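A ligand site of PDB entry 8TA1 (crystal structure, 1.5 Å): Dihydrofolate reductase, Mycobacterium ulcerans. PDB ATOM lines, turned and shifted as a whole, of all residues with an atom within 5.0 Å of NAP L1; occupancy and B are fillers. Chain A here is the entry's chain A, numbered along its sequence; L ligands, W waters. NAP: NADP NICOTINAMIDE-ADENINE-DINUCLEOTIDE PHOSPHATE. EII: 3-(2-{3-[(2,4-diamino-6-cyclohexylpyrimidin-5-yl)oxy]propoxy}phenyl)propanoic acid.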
ATOM      1  N   ILE A  15      18.381 -17.404  22.000  1.00  0.00           N
ATOM      2  CA  ILE A  15      17.225 -17.708  21.166  1.00  0.00           C
ATOM      3  C   ILE A  15      16.256 -18.503  22.029  1.00  0.00           C
ATOM      4  O   ILE A  15      16.672 -19.458  22.702  1.00  0.00           O
ATOM      5  CB  ILE A  15      17.630 -18.435  19.860  1.00  0.00           C
ATOM      6  CG1 ILE A  15      16.399 -18.710  19.012  1.00  0.00           C
ATOM      7  CG2 ILE A  15      18.433 -19.686  20.142  1.00  0.00           C
ATOM      8  CD1 ILE A  15      16.750 -19.116  17.576  1.00  0.00           C
ATOM      9  N   TRP A  16      15.007 -18.055  22.074  1.00  0.00           N
ATOM     10  CA  TRP A  16      13.972 -18.757  22.817  1.00  0.00           C
ATOM     11  C   TRP A  16      12.607 -18.487  22.200  1.00  0.00           C
ATOM     12  O   TRP A  16      12.414 -17.531  21.443  1.00  0.00           O
ATOM     13  CB  TRP A  16      13.935 -18.375  24.303  1.00  0.00           C
ATOM     14  CG  TRP A  16      13.384 -17.023  24.694  1.00  0.00           C
ATOM     15  CD1 TRP A  16      12.068 -16.703  24.952  1.00  0.00           C
ATOM     16  CD2 TRP A  16      14.132 -15.832  24.954  1.00  0.00           C
ATOM     17  NE1 TRP A  16      11.970 -15.395  25.353  1.00  0.00           N
ATOM     18  CE2 TRP A  16      13.224 -14.835  25.380  1.00  0.00           C
ATOM     19  CE3 TRP A  16      15.504 -15.512  24.891  1.00  0.00           C
ATOM     20  CZ2 TRP A  16      13.626 -13.538  25.694  1.00  0.00           C
ATOM     21  CZ3 TRP A  16      15.898 -14.221  25.206  1.00  0.00           C
ATOM     22  CH2 TRP A  16      14.963 -13.255  25.615  1.00  0.00           C
ATOM     23  N   ALA A  17      11.659 -19.363  22.535  1.00  0.00           N
ATOM     24  CA  ALA A  17      10.231 -19.216  22.215  1.00  0.00           C
ATOM     25  C   ALA A  17       9.456 -19.169  23.534  1.00  0.00           C
ATOM     26  O   ALA A  17       9.654 -20.026  24.398  1.00  0.00           O
ATOM     27  CB  ALA A  17       9.782 -20.393  21.389  1.00  0.00           C
ATOM     28  N   ILE A  24       8.368 -20.683  28.974  1.00  0.00           N
ATOM     29  CA  ILE A  24       9.159 -21.409  27.982  1.00  0.00           C
ATOM     30  C   ILE A  24       9.137 -22.929  28.153  1.00  0.00           C
ATOM     31  O   ILE A  24       9.410 -23.642  27.170  1.00  0.00           O
ATOM     32  CB  ILE A  24      10.624 -20.917  27.892  1.00  0.00           C
ATOM     33  CG1 ILE A  24      11.431 -21.323  29.139  1.00  0.00           C
ATOM     34  CG2 ILE A  24      10.653 -19.415  27.589  1.00  0.00           C
ATOM     35  CD1 ILE A  24      12.946 -21.046  28.980  1.00  0.00           C
ATOM     36  N   GLY A  25       8.851 -23.436  29.339  1.00  0.00           N
ATOM     37  CA  GLY A  25       8.950 -24.861  29.589  1.00  0.00           C
ATOM     38  C   GLY A  25       7.993 -25.314  30.672  1.00  0.00           C
ATOM     39  O   GLY A  25       7.677 -24.566  31.603  1.00  0.00           O
ATOM     40  N   ARG A  26       7.573 -26.557  30.551  1.00  0.00           N
ATOM     41  CA  ARG A  26       6.678 -27.178  31.532  1.00  0.00           C
ATOM     42  C   ARG A  26       6.845 -28.684  31.425  1.00  0.00           C
ATOM     43  O   ARG A  26       6.899 -29.223  30.317  1.00  0.00           O
ATOM     44  CB  ARG A  26       5.220 -26.780  31.239  1.00  0.00           C
ATOM     45  CG  ARG A  26       4.218 -27.499  32.113  1.00  0.00           C
ATOM     46  CD  ARG A  26       2.787 -27.034  31.879  1.00  0.00           C
ATOM     47  NE  ARG A  26       2.631 -25.637  32.250  1.00  0.00           N
ATOM     48  CZ  ARG A  26       1.543 -24.912  32.010  1.00  0.00           C
ATOM     49  NH1 ARG A  26       0.494 -25.436  31.390  1.00  0.00           N
ATOM     50  NH2 ARG A  26       1.509 -23.654  32.398  1.00  0.00           N
ATOM     51  N   GLY A  28       9.242 -30.685  31.770  1.00  0.00           N
ATOM     52  CA  GLY A  28      10.389 -31.151  31.022  1.00  0.00           C
ATOM     53  C   GLY A  28      10.268 -31.040  29.510  1.00  0.00           C
ATOM     54  O   GLY A  28      11.025 -31.687  28.786  1.00  0.00           O
ATOM     55  N   GLY A  29       9.324 -30.242  29.017  1.00  0.00           N
ATOM     56  CA  GLY A  29       9.176 -30.026  27.593  1.00  0.00           C
ATOM     57  C   GLY A  29       8.595 -28.653  27.305  1.00  0.00           C
ATOM     58  O   GLY A  29       8.659 -27.747  28.154  1.00  0.00           O
ATOM     59  N   ILE A  30       8.021 -28.509  26.119  1.00  0.00           N
ATOM     60  CA  ILE A  30       7.501 -27.248  25.590  1.00  0.00           C
ATOM     61  C   ILE A  30       5.988 -27.416  25.497  1.00  0.00           C
ATOM     62  O   ILE A  30       5.518 -28.312  24.799  1.00  0.00           O
ATOM     63  CB  ILE A  30       8.040 -26.950  24.183  1.00  0.00           C
ATOM     64  CG1 ILE A  30       9.562 -27.165  24.104  1.00  0.00           C
ATOM     65  CG2 ILE A  30       7.629 -25.528  23.773  1.00  0.00           C
ATOM     66  CD1 ILE A  30      10.304 -26.159  24.833  1.00  0.00           C
ATOM     67  N   TRP A  32       3.435 -26.280  23.896  1.00  0.00           N
ATOM     68  CA  TRP A  32       2.674 -25.963  22.700  1.00  0.00           C
ATOM     69  C   TRP A  32       3.427 -26.572  21.533  1.00  0.00           C
ATOM     70  O   TRP A  32       4.579 -26.980  21.668  1.00  0.00           O
ATOM     71  CB  TRP A  32       2.522 -24.449  22.495  1.00  0.00           C
ATOM     72  CG  TRP A  32       3.834 -23.767  22.342  1.00  0.00           C
ATOM     73  CD1 TRP A  32       4.577 -23.694  21.202  1.00  0.00           C
ATOM     74  CD2 TRP A  32       4.593 -23.104  23.350  1.00  0.00           C
ATOM     75  NE1 TRP A  32       5.748 -23.030  21.435  1.00  0.00           N
ATOM     76  CE2 TRP A  32       5.785 -22.656  22.757  1.00  0.00           C
ATOM     77  CE3 TRP A  32       4.380 -22.847  24.703  1.00  0.00           C
ATOM     78  CZ2 TRP A  32       6.766 -21.957  23.476  1.00  0.00           C
ATOM     79  CZ3 TRP A  32       5.336 -22.149  25.406  1.00  0.00           C
ATOM     80  CH2 TRP A  32       6.524 -21.714  24.795  1.00  0.00           C
ATOM     81  N   GLY A  53      21.729 -25.665  29.016  1.00  0.00           N
ATOM     82  CA  GLY A  53      21.815 -26.300  30.310  1.00  0.00           C
ATOM     83  C   GLY A  53      21.528 -27.791  30.224  1.00  0.00           C
ATOM     84  O   GLY A  53      20.880 -28.298  29.294  1.00  0.00           O
ATOM     85  N   ARG A  54      21.958 -28.495  31.267  1.00  0.00           N
ATOM     86  CA  ARG A  54      21.809 -29.943  31.291  1.00  0.00           C
ATOM     87  C   ARG A  54      20.334 -30.366  31.260  1.00  0.00           C
ATOM     88  O   ARG A  54      20.001 -31.368  30.624  1.00  0.00           O
ATOM     89  CB  ARG A  54      22.556 -30.537  32.481  1.00  0.00           C
ATOM     90  CG  ARG A  54      22.780 -32.048  32.410  1.00  0.00           C
ATOM     91  CD  ARG A  54      21.604 -32.843  32.972  1.00  0.00           C
ATOM     92  NE  ARG A  54      21.286 -32.419  34.333  1.00  0.00           N
ATOM     93  CZ  ARG A  54      20.082 -32.480  34.891  1.00  0.00           C
ATOM     94  NH1 ARG A  54      19.046 -33.035  34.274  1.00  0.00           N
ATOM     95  NH2 ARG A  54      19.888 -31.917  36.081  1.00  0.00           N
ATOM     96  N   ARG A  55      19.434 -29.608  31.885  1.00  0.00           N
ATOM     97  CA  ARG A  55      18.023 -30.018  31.830  1.00  0.00           C
ATOM     98  C   ARG A  55      17.465 -29.894  30.417  1.00  0.00           C
ATOM     99  O   ARG A  55      16.663 -30.736  29.977  1.00  0.00           O
ATOM    100  CB  ARG A  55      17.188 -29.233  32.847  1.00  0.00           C
ATOM    101  CG  ARG A  55      17.481 -29.585  34.292  1.00  0.00           C
ATOM    102  CD  ARG A  55      16.725 -28.691  35.288  1.00  0.00           C
ATOM    103  NE  ARG A  55      15.292 -28.645  35.076  1.00  0.00           N
ATOM    104  CZ  ARG A  55      14.411 -29.552  35.489  1.00  0.00           C
ATOM    105  NH1 ARG A  55      14.790 -30.620  36.192  1.00  0.00           N
ATOM    106  NH2 ARG A  55      13.118 -29.364  35.226  1.00  0.00           N
ATOM    107  N   THR A  56      17.872 -28.860  29.672  1.00  0.00           N
ATOM    108  CA  THR A  56      17.471 -28.740  28.271  1.00  0.00           C
ATOM    109  C   THR A  56      18.042 -29.906  27.446  1.00  0.00           C
ATOM    110  O   THR A  56      17.316 -30.498  26.636  1.00  0.00           O
ATOM    111  CB  THR A  56      17.889 -27.381  27.719  1.00  0.00           C
ATOM    112  OG1 THR A  56      17.141 -26.346  28.347  1.00  0.00           O
ATOM    113  CG2 THR A  56      17.600 -27.299  26.225  1.00  0.00           C
ATOM    114  N   SER A  59      15.882 -32.698  27.927  1.00  0.00           N
ATOM    115  CA  SER A  59      14.553 -32.469  27.363  1.00  0.00           C
ATOM    116  C   SER A  59      14.476 -32.756  25.865  1.00  0.00           C
ATOM    117  O   SER A  59      13.368 -32.824  25.317  1.00  0.00           O
ATOM    118  CB  SER A  59      14.094 -31.018  27.611  1.00  0.00           C
ATOM    119  OG  SER A  59      14.661 -30.087  26.707  1.00  0.00           O
ATOM    120  N   VAL A  75      26.061 -27.477  29.586  1.00  0.00           N
ATOM    121  CA  VAL A  75      26.561 -26.905  30.829  1.00  0.00           C
ATOM    122  C   VAL A  75      25.978 -27.683  32.012  1.00  0.00           C
ATOM    123  O   VAL A  75      24.749 -27.757  32.171  1.00  0.00           O
ATOM    124  CB  VAL A  75      26.198 -25.409  30.931  1.00  0.00           C
ATOM    125  CG1 VAL A  75      26.763 -24.820  32.214  1.00  0.00           C
ATOM    126  CG2 VAL A  75      26.696 -24.657  29.696  1.00  0.00           C
ATOM    127  N   THR A  76      26.852 -28.186  32.875  1.00  0.00           N
ATOM    128  CA  THR A  76      26.477 -28.988  34.033  1.00  0.00           C
ATOM    129  C   THR A  76      27.499 -28.752  35.141  1.00  0.00           C
ATOM    130  O   THR A  76      28.656 -28.415  34.879  1.00  0.00           O
ATOM    131  CB  THR A  76      26.429 -30.481  33.664  1.00  0.00           C
ATOM    132  OG1 THR A  76      26.042 -31.287  34.778  1.00  0.00           O
ATOM    133  CG2 THR A  76      27.790 -30.957  33.188  1.00  0.00           C
ATOM    134  N   ARG A  77      27.069 -29.007  36.374  1.00  0.00           N
ATOM    135  CA  ARG A  77      28.003 -29.113  37.492  1.00  0.00           C
ATOM    136  C   ARG A  77      28.451 -30.545  37.741  1.00  0.00           C
ATOM    137  O   ARG A  77      29.293 -30.796  38.609  1.00  0.00           O
ATOM    138  CB  ARG A  77      27.394 -28.532  38.784  1.00  0.00           C
ATOM    139  CG  ARG A  77      27.104 -27.044  38.721  1.00  0.00           C
ATOM    140  CD  ARG A  77      26.738 -26.507  40.110  1.00  0.00           C
ATOM    141  NE  ARG A  77      26.472 -25.080  40.083  1.00  0.00           N
ATOM    142  CZ  ARG A  77      25.305 -24.516  39.816  1.00  0.00           C
ATOM    143  NH1 ARG A  77      24.247 -25.234  39.485  1.00  0.00           N
ATOM    144  NH2 ARG A  77      25.194 -23.197  39.900  1.00  0.00           N
ATOM    145  N   GLN A  78      27.898 -31.515  37.028  1.00  0.00           N
ATOM    146  CA  GLN A  78      28.282 -32.904  37.217  1.00  0.00           C
ATOM    147  C   GLN A  78      29.582 -33.174  36.478  1.00  0.00           C
ATOM    148  O   GLN A  78      29.582 -33.344  35.257  1.00  0.00           O
ATOM    149  CB  GLN A  78      27.182 -33.824  36.720  1.00  0.00           C
ATOM    150  CG  GLN A  78      25.852 -33.635  37.372  1.00  0.00           C
ATOM    151  CD  GLN A  78      24.858 -34.616  36.799  1.00  0.00           C
ATOM    152  OE1 GLN A  78      25.018 -35.834  36.949  1.00  0.00           O
ATOM    153  NE2 GLN A  78      23.848 -34.104  36.120  1.00  0.00           N
ATOM    154  N   GLY A  90      31.685 -27.140  32.387  1.00  0.00           N
ATOM    155  CA  GLY A  90      31.274 -26.937  33.760  1.00  0.00           C
ATOM    156  C   GLY A  90      30.772 -25.554  34.108  1.00  0.00           C
ATOM    157  O   GLY A  90      30.479 -25.288  35.280  1.00  0.00           O
ATOM    158  N   SER A  91      30.690 -24.658  33.135  1.00  0.00           N
ATOM    159  CA  SER A  91      30.186 -23.311  33.387  1.00  0.00           C
ATOM    160  C   SER A  91      29.832 -22.662  32.056  1.00  0.00           C
ATOM    161  O   SER A  91      30.308 -23.056  30.996  1.00  0.00           O
ATOM    162  CB  SER A  91      31.228 -22.432  34.091  1.00  0.00           C
ATOM    163  OG  SER A  91      32.267 -22.089  33.179  1.00  0.00           O
ATOM    164  N   ILE A 108      20.690 -21.620  23.883  1.00  0.00           N
ATOM    165  CA  ILE A 108      19.395 -22.138  23.480  1.00  0.00           C
ATOM    166  C   ILE A 108      18.547 -22.576  24.667  1.00  0.00           C
ATOM    167  O   ILE A 108      17.516 -23.221  24.467  1.00  0.00           O
ATOM    168  CB  ILE A 108      19.534 -23.270  22.427  1.00  0.00           C
ATOM    169  CG1 ILE A 108      20.198 -24.515  23.033  1.00  0.00           C
ATOM    170  CG2 ILE A 108      20.318 -22.784  21.221  1.00  0.00           C
ATOM    171  CD1 ILE A 108      19.916 -25.757  22.220  1.00  0.00           C
ATOM    172  N   GLY A 109      18.948 -22.253  25.876  1.00  0.00           N
ATOM    173  CA  GLY A 109      18.132 -22.456  27.066  1.00  0.00           C
ATOM    174  C   GLY A 109      18.813 -23.402  28.048  1.00  0.00           C
ATOM    175  O   GLY A 109      19.914 -23.902  27.807  1.00  0.00           O
ATOM    176  N   GLY A 110      18.148 -23.640  29.173  1.00  0.00           N
ATOM    177  CA  GLY A 110      16.828 -23.143  29.543  1.00  0.00           C
ATOM    178  C   GLY A 110      16.851 -21.893  30.375  1.00  0.00           C
ATOM    179  O   GLY A 110      17.733 -21.081  30.241  1.00  0.00           O
ATOM    180  N   ALA A 111      15.839 -21.755  31.239  1.00  0.00           N
ATOM    181  CA  ALA A 111      15.709 -20.540  32.030  1.00  0.00           C
ATOM    182  C   ALA A 111      16.920 -20.271  32.897  1.00  0.00           C
ATOM    183  O   ALA A 111      17.348 -19.117  33.050  1.00  0.00           O
ATOM    184  CB  ALA A 111      14.452 -20.623  32.907  1.00  0.00           C
ATOM    185  N   GLN A 112      17.471 -21.304  33.528  1.00  0.00           N
ATOM    186  CA  GLN A 112      18.639 -21.079  34.379  1.00  0.00           C
ATOM    187  C   GLN A 112      19.805 -20.517  33.559  1.00  0.00           C
ATOM    188  O   GLN A 112      20.474 -19.570  33.981  1.00  0.00           O
ATOM    189  CB  GLN A 112      19.077 -22.368  35.093  1.00  0.00           C
ATOM    190  CG  GLN A 112      18.007 -23.053  35.898  1.00  0.00           C
ATOM    191  CD  GLN A 112      18.566 -24.179  36.744  1.00  0.00           C
ATOM    192  OE1 GLN A 112      19.764 -24.211  37.032  1.00  0.00           O
ATOM    193  NE2 GLN A 112      17.714 -25.091  37.154  1.00  0.00           N
ATOM    194  N   ILE A 113      20.064 -21.112  32.394  1.00  0.00           N
ATOM    195  CA  ILE A 113      21.210 -20.686  31.583  1.00  0.00           C
ATOM    196  C   ILE A 113      20.954 -19.334  30.918  1.00  0.00           C
ATOM    197  O   ILE A 113      21.877 -18.525  30.793  1.00  0.00           O
ATOM    198  CB  ILE A 113      21.600 -21.764  30.563  1.00  0.00           C
ATOM    199  CG1 ILE A 113      22.105 -23.045  31.214  1.00  0.00           C
ATOM    200  CG2 ILE A 113      22.648 -21.224  29.587  1.00  0.00           C
ATOM    201  CD1 ILE A 113      22.931 -22.940  32.432  1.00  0.00           C
ATOM    202  N   TYR A 114      19.709 -19.037  30.520  1.00  0.00           N
ATOM    203  CA  TYR A 114      19.455 -17.715  29.929  1.00  0.00           C
ATOM    204  C   TYR A 114      19.849 -16.621  30.900  1.00  0.00           C
ATOM    205  O   TYR A 114      20.376 -15.585  30.490  1.00  0.00           O
ATOM    206  CB  TYR A 114      17.990 -17.510  29.539  1.00  0.00           C
ATOM    207  CG  TYR A 114      17.500 -18.271  28.340  1.00  0.00           C
ATOM    208  CD1 TYR A 114      18.240 -18.345  27.162  1.00  0.00           C
ATOM    209  CD2 TYR A 114      16.291 -18.948  28.394  1.00  0.00           C
ATOM    210  CE1 TYR A 114      17.760 -19.061  26.068  1.00  0.00           C
ATOM    211  CE2 TYR A 114      15.828 -19.685  27.310  1.00  0.00           C
ATOM    212  CZ  TYR A 114      16.564 -19.736  26.157  1.00  0.00           C
ATOM    213  OH  TYR A 114      16.094 -20.477  25.105  1.00  0.00           O
ATOM    214  N   LEU A 116      22.119 -16.546  33.198  1.00  0.00           N
ATOM    215  CA  LEU A 116      23.559 -16.402  33.252  1.00  0.00           C
ATOM    216  C   LEU A 116      24.113 -15.806  31.974  1.00  0.00           C
ATOM    217  O   LEU A 116      25.152 -15.117  31.999  1.00  0.00           O
ATOM    218  CB  LEU A 116      24.207 -17.783  33.471  1.00  0.00           C
ATOM    219  CG  LEU A 116      23.787 -18.519  34.749  1.00  0.00           C
ATOM    220  CD1 LEU A 116      24.483 -19.859  34.835  1.00  0.00           C
ATOM    221  CD2 LEU A 116      24.098 -17.659  35.964  1.00  0.00           C
ATOM    222  N   ALA A 140       9.185 -23.098  33.613  1.00  0.00           N
ATOM    223  CA  ALA A 140      10.370 -22.325  33.350  1.00  0.00           C
ATOM    224  C   ALA A 140       9.943 -21.104  32.563  1.00  0.00           C
ATOM    225  O   ALA A 140       9.130 -21.221  31.630  1.00  0.00           O
ATOM    226  CB  ALA A 140      11.393 -23.139  32.553  1.00  0.00           C
HETATM  227  PA  NAP L   1      18.385 -25.503  32.101  1.00  0.00           P
HETATM  228  O1A NAP L   1      18.749 -24.073  32.245  1.00  0.00           O
HETATM  229  O2A NAP L   1      18.270 -26.090  30.727  1.00  0.00           O
HETATM  230  O5B NAP L   1      19.441 -26.490  32.863  1.00  0.00           O
HETATM  231  C5B NAP L   1      19.746 -26.277  34.229  1.00  0.00           C
HETATM  232  C4B NAP L   1      20.995 -27.073  34.536  1.00  0.00           C
HETATM  233  O4B NAP L   1      22.123 -26.374  34.050  1.00  0.00           O
HETATM  234  C3B NAP L   1      21.241 -27.279  36.041  1.00  0.00           C
HETATM  235  O3B NAP L   1      20.456 -28.299  36.598  1.00  0.00           O
HETATM  236  C2B NAP L   1      22.754 -27.577  35.978  1.00  0.00           C
HETATM  237  O2B NAP L   1      22.965 -28.829  35.452  1.00  0.00           O
HETATM  238  C1B NAP L   1      23.213 -26.568  34.907  1.00  0.00           C
HETATM  239  N9A NAP L   1      23.629 -25.305  35.461  1.00  0.00           N
HETATM  240  C8A NAP L   1      22.867 -24.236  35.850  1.00  0.00           C
HETATM  241  N7A NAP L   1      23.607 -23.263  36.321  1.00  0.00           N
HETATM  242  C5A NAP L   1      24.901 -23.706  36.240  1.00  0.00           C
HETATM  243  C6A NAP L   1      26.166 -23.172  36.556  1.00  0.00           C
HETATM  244  N6A NAP L   1      26.313 -21.941  37.066  1.00  0.00           N
HETATM  245  N1A NAP L   1      27.260 -23.905  36.328  1.00  0.00           N
HETATM  246  C2A NAP L   1      27.120 -25.130  35.817  1.00  0.00           C
HETATM  247  N3A NAP L   1      26.002 -25.740  35.470  1.00  0.00           N
HETATM  248  C4A NAP L   1      24.934 -24.974  35.693  1.00  0.00           C
HETATM  249  O3  NAP L   1      17.040 -25.866  32.946  1.00  0.00           O
HETATM  250  PN  NAP L   1      15.594 -25.146  33.054  1.00  0.00           P
HETATM  251  O1N NAP L   1      15.743 -23.705  33.375  1.00  0.00           O
HETATM  252  O2N NAP L   1      14.813 -26.049  33.948  1.00  0.00           O
HETATM  253  O5D NAP L   1      15.011 -25.241  31.548  1.00  0.00           O
HETATM  254  C5D NAP L   1      14.487 -26.430  31.012  1.00  0.00           C
HETATM  255  C4D NAP L   1      13.050 -26.234  30.555  1.00  0.00           C
HETATM  256  O4D NAP L   1      13.055 -25.208  29.536  1.00  0.00           O
HETATM  257  C3D NAP L   1      12.432 -27.456  29.914  1.00  0.00           C
HETATM  258  O3D NAP L   1      11.039 -27.399  30.103  1.00  0.00           O
HETATM  259  C2D NAP L   1      12.697 -27.237  28.434  1.00  0.00           C
HETATM  260  O2D NAP L   1      11.798 -27.903  27.592  1.00  0.00           O
HETATM  261  C1D NAP L   1      12.496 -25.732  28.372  1.00  0.00           C
HETATM  262  N1N NAP L   1      13.114 -25.012  27.238  1.00  0.00           N
HETATM  263  C2N NAP L   1      12.381 -24.195  26.470  1.00  0.00           C
HETATM  264  C3N NAP L   1      12.935 -23.466  25.459  1.00  0.00           C
HETATM  265  C7N NAP L   1      12.047 -22.599  24.654  1.00  0.00           C
HETATM  266  O7N NAP L   1      10.802 -22.627  24.709  1.00  0.00           O
HETATM  267  N7N NAP L   1      12.703 -21.786  23.893  1.00  0.00           N
HETATM  268  C4N NAP L   1      14.308 -23.599  25.205  1.00  0.00           C
HETATM  269  C5N NAP L   1      15.069 -24.448  26.031  1.00  0.00           C
HETATM  270  C6N NAP L   1      14.450 -25.126  27.055  1.00  0.00           C
HETATM  271  P2B NAP L   1      23.227 -30.126  36.520  1.00  0.00           P
HETATM  272  O1X NAP L   1      23.537 -31.275  35.571  1.00  0.00           O
HETATM  273  O2X NAP L   1      24.413 -29.712  37.387  1.00  0.00           O
HETATM  274  O3X NAP L   1      21.935 -30.301  37.324  1.00  0.00           O
HETATM  275  C15 EII L   2      15.688 -25.391  21.489  1.00  0.00           C
HETATM  276  C11 EII L   2      13.703 -28.927  20.644  1.00  0.00           C
HETATM  277  C10 EII L   2      12.633 -29.202  21.494  1.00  0.00           C
HETATM  278  C13 EII L   2      14.780 -27.564  22.342  1.00  0.00           C
HETATM  279  C14 EII L   2      15.926 -26.569  22.448  1.00  0.00           C
HETATM  280  C02 EII L   2      16.060 -29.174  16.225  1.00  0.00           C
HETATM  281  C04 EII L   2      14.756 -29.337  16.990  1.00  0.00           C
HETATM  282  C05 EII L   2      14.944 -29.146  18.447  1.00  0.00           C
HETATM  283  C06 EII L   2      13.773 -29.436  19.346  1.00  0.00           C
HETATM  284  C07 EII L   2      12.724 -30.238  18.916  1.00  0.00           C
HETATM  285  C08 EII L   2      11.632 -30.552  19.754  1.00  0.00           C
HETATM  286  C09 EII L   2      11.579 -30.033  21.041  1.00  0.00           C
HETATM  287  C17 EII L   2      14.213 -23.534  21.296  1.00  0.00           C
HETATM  288  C18 EII L   2      14.849 -22.292  21.397  1.00  0.00           C
HETATM  289  C21 EII L   2      13.350 -21.395  19.877  1.00  0.00           C
HETATM  290  C24 EII L   2      13.099 -23.664  20.467  1.00  0.00           C
HETATM  291  C25 EII L   2      12.320 -24.956  20.278  1.00  0.00           C
HETATM  292  C26 EII L   2      10.865 -24.818  20.728  1.00  0.00           C
HETATM  293  C27 EII L   2      10.062 -26.101  20.456  1.00  0.00           C
HETATM  294  C28 EII L   2      10.108 -26.574  19.023  1.00  0.00           C
HETATM  295  C29 EII L   2      11.524 -26.681  18.533  1.00  0.00           C
HETATM  296  C30 EII L   2      12.356 -25.419  18.797  1.00  0.00           C
HETATM  297  N19 EII L   2      15.934 -22.126  22.208  1.00  0.00           N
HETATM  298  N20 EII L   2      14.447 -21.212  20.674  1.00  0.00           N
HETATM  299  N22 EII L   2      12.915 -20.322  19.139  1.00  0.00           N
HETATM  300  N23 EII L   2      12.668 -22.579  19.747  1.00  0.00           N
HETATM  301  O01 EII L   2      16.527 -28.011  16.082  1.00  0.00           O
HETATM  302  O03 EII L   2      16.655 -30.212  15.781  1.00  0.00           O
HETATM  303  O12 EII L   2      14.765 -28.144  21.040  1.00  0.00           O
HETATM  304  O16 EII L   2      14.637 -24.606  22.053  1.00  0.00           O
HETATM  305  O   HOH W   1      22.626 -21.190  37.746  1.00  0.00           O
HETATM  306  O   HOH W   2      28.262 -20.093  38.211  1.00  0.00           O
HETATM  307  O   HOH W   3      13.360 -29.814  32.171  1.00  0.00           O
HETATM  308  O   HOH W   4      12.914 -28.737  25.252  1.00  0.00           O
HETATM  309  O   HOH W   5      24.974 -31.355  39.652  1.00  0.00           O
HETATM  310  O   HOH W   6      23.844 -28.277  39.519  1.00  0.00           O
HETATM  311  O   HOH W   7      12.201 -26.692  34.133  1.00  0.00           O
HETATM  312  O   HOH W   8      10.160 -27.992  32.657  1.00  0.00           O
HETATM  313  O   HOH W   9      18.724 -27.331  38.659  1.00  0.00           O
HETATM  314  O   HOH W  10      14.810 -25.438  36.719  1.00  0.00           O
HETATM  315  O   HOH W  11      29.824 -23.388  37.378  1.00  0.00           O
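Water W6 bridges an oxygen (O2X) of NAP L1 (2.6 Å) and the guanidinium group (NH1) of Arg 77 (3.1 Å). Water W7 lies within hydrogen-bond range of an oxygen (O2N) of NAP L1 and the guanidinium group of Arg 55. Water W4 lies within hydrogen-bond range of the side-chain hydroxyl of Ser 59 and an oxygen (O2D) of NAP L1. Water W8 bridges O3D of NAP L1 (2.8 Å) and N of Gly 28 (3.0 Å). Water W10 bridges O2N of NAP L1 and NE2 of Gln 112. Water W9 bridges O3B of NAP L1 (2.9 Å) and NE2 of Gln 112 (2.9 Å).
The side-chain hydroxyl (OG1) of Thr 76 is in hydrogen-bond range of an oxygen (O1X) of NAP L1, at 2.6 Å. O2A of NAP L1 is in hydrogen-bond range of N of Thr 56, at 3.0 Å. O2A of NAP L1 lies within hydrogen-bond range of OG1 of Thr 56 (2.6 Å). The guanidinium group of Arg 54 lies within salt-bridge range of an oxygen (O1X) of NAP L1, at 2.8 Å. The backbone NH (N) of Arg 55 is in hydrogen-bond range of an oxygen (O5B) of NAP L1 (3.3 Å). An oxygen (O2N) of NAP L1 is in salt-bridge range of the guanidinium group (NE) of Arg 55 (2.9 Å). O1N of NAP L1 lies within hydrogen-bond range of N of Ala 111 (2.9 Å). An oxygen (O1X) of NAP L1 lies within hydrogen-bond range of the side-chain amide nitrogen of Gln 78 (2.9 Å). The backbone NH (N) of Gly 110 sits at hydrogen-bond distance from an oxygen (O2A) of NAP L1 (2.9 Å). The backbone NH (N) of Arg 77 is in hydrogen-bond range of an oxygen (O2X) of NAP L1 (2.9 Å). An oxygen (O1N) of NAP L1 lies within hydrogen-bond range of the backbone NH of Gln 112 (3.0 Å). N of Gly 29 lies within hydrogen-bond range of O3D of NAP L1 (3.5 Å). O of Gly 29 lies within hydrogen-bond range of O3D of NAP L1 (3.1 Å). An oxygen (O1A) of NAP L1 lies within hydrogen-bond range of the backbone NH of Ile 113, 3.2 Å away. The backbone carbonyl oxygen of Ile 108 is in hydrogen-bond range of a nitrogen (N19) of EII L2, at 3.0 Å. N of Trp 16 lies close to N20 of EII L2, 3.5 Å away. The side-chain hydroxyl of Tyr 114 lies within hydrogen-bond range of a nitrogen (N19) of EII L2 (3.3 Å). The backbone carbonyl oxygen (O) of Ile 15 sits at hydrogen-bond distance from a nitrogen (N19) of EII L2 (2.8 Å).
O of Ala 17 lies close to O7N of NAP L1, at 2.9 Å. O of Ile 24 lies close to O7N of NAP L1, 3.0 Å away. CA of Trp 16 touches N7N of NAP L1, 3.5 Å away. Gly 25 touches NAP L1. N of Arg 26 touches O3D of NAP L1 (3.6 Å). Gly 28 touches NAP L1 (C to O3D, 3.8 Å). CD1 of Ile 30 touches C2N of NAP L1, at 3.3 Å. Gly 53 touches NAP L1 (CA to O5B, 3.5 Å). Ser 59 touches NAP L1. O of Val 75 touches C1B of NAP L1, at 3.4 Å. Gly 90 touches NAP L1. Ile 108 touches NAP L1 (O to C5N, 3.2 Å). Gly 109 touches NAP L1. Tyr 114 touches NAP L1 (OH to C4N, 3.6 Å). Leu 116 touches NAP L1.
OG1 of Thr 76 lies within hydrogen-bond range of N of Gln 78 (2.9 Å). OG1 of Thr 56 is in hydrogen-bond range of N of Gly 110. The side-chain hydroxyl (OG) of Ser 59 sits at hydrogen-bond distance from the backbone carbonyl oxygen (O) of Thr 56 (2.7 Å). N of Arg 54 lies within hydrogen-bond range of O of Val 75, 3.0 Å away. The backbone NH (N) of Ile 24 sits at hydrogen-bond distance from the backbone carbonyl oxygen (O) of Ala 140, 2.8 Å away. The backbone carbonyl oxygen (O) of Ile 108 sits at hydrogen-bond distance from the side-chain hydroxyl (OH) of Tyr 114. The backbone carbonyl oxygen (O) of Gly 25 lies within hydrogen-bond range of the backbone NH (N) of Ala 140. N of Gly 109 sits close to OH of Tyr 114 (3.4 Å).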
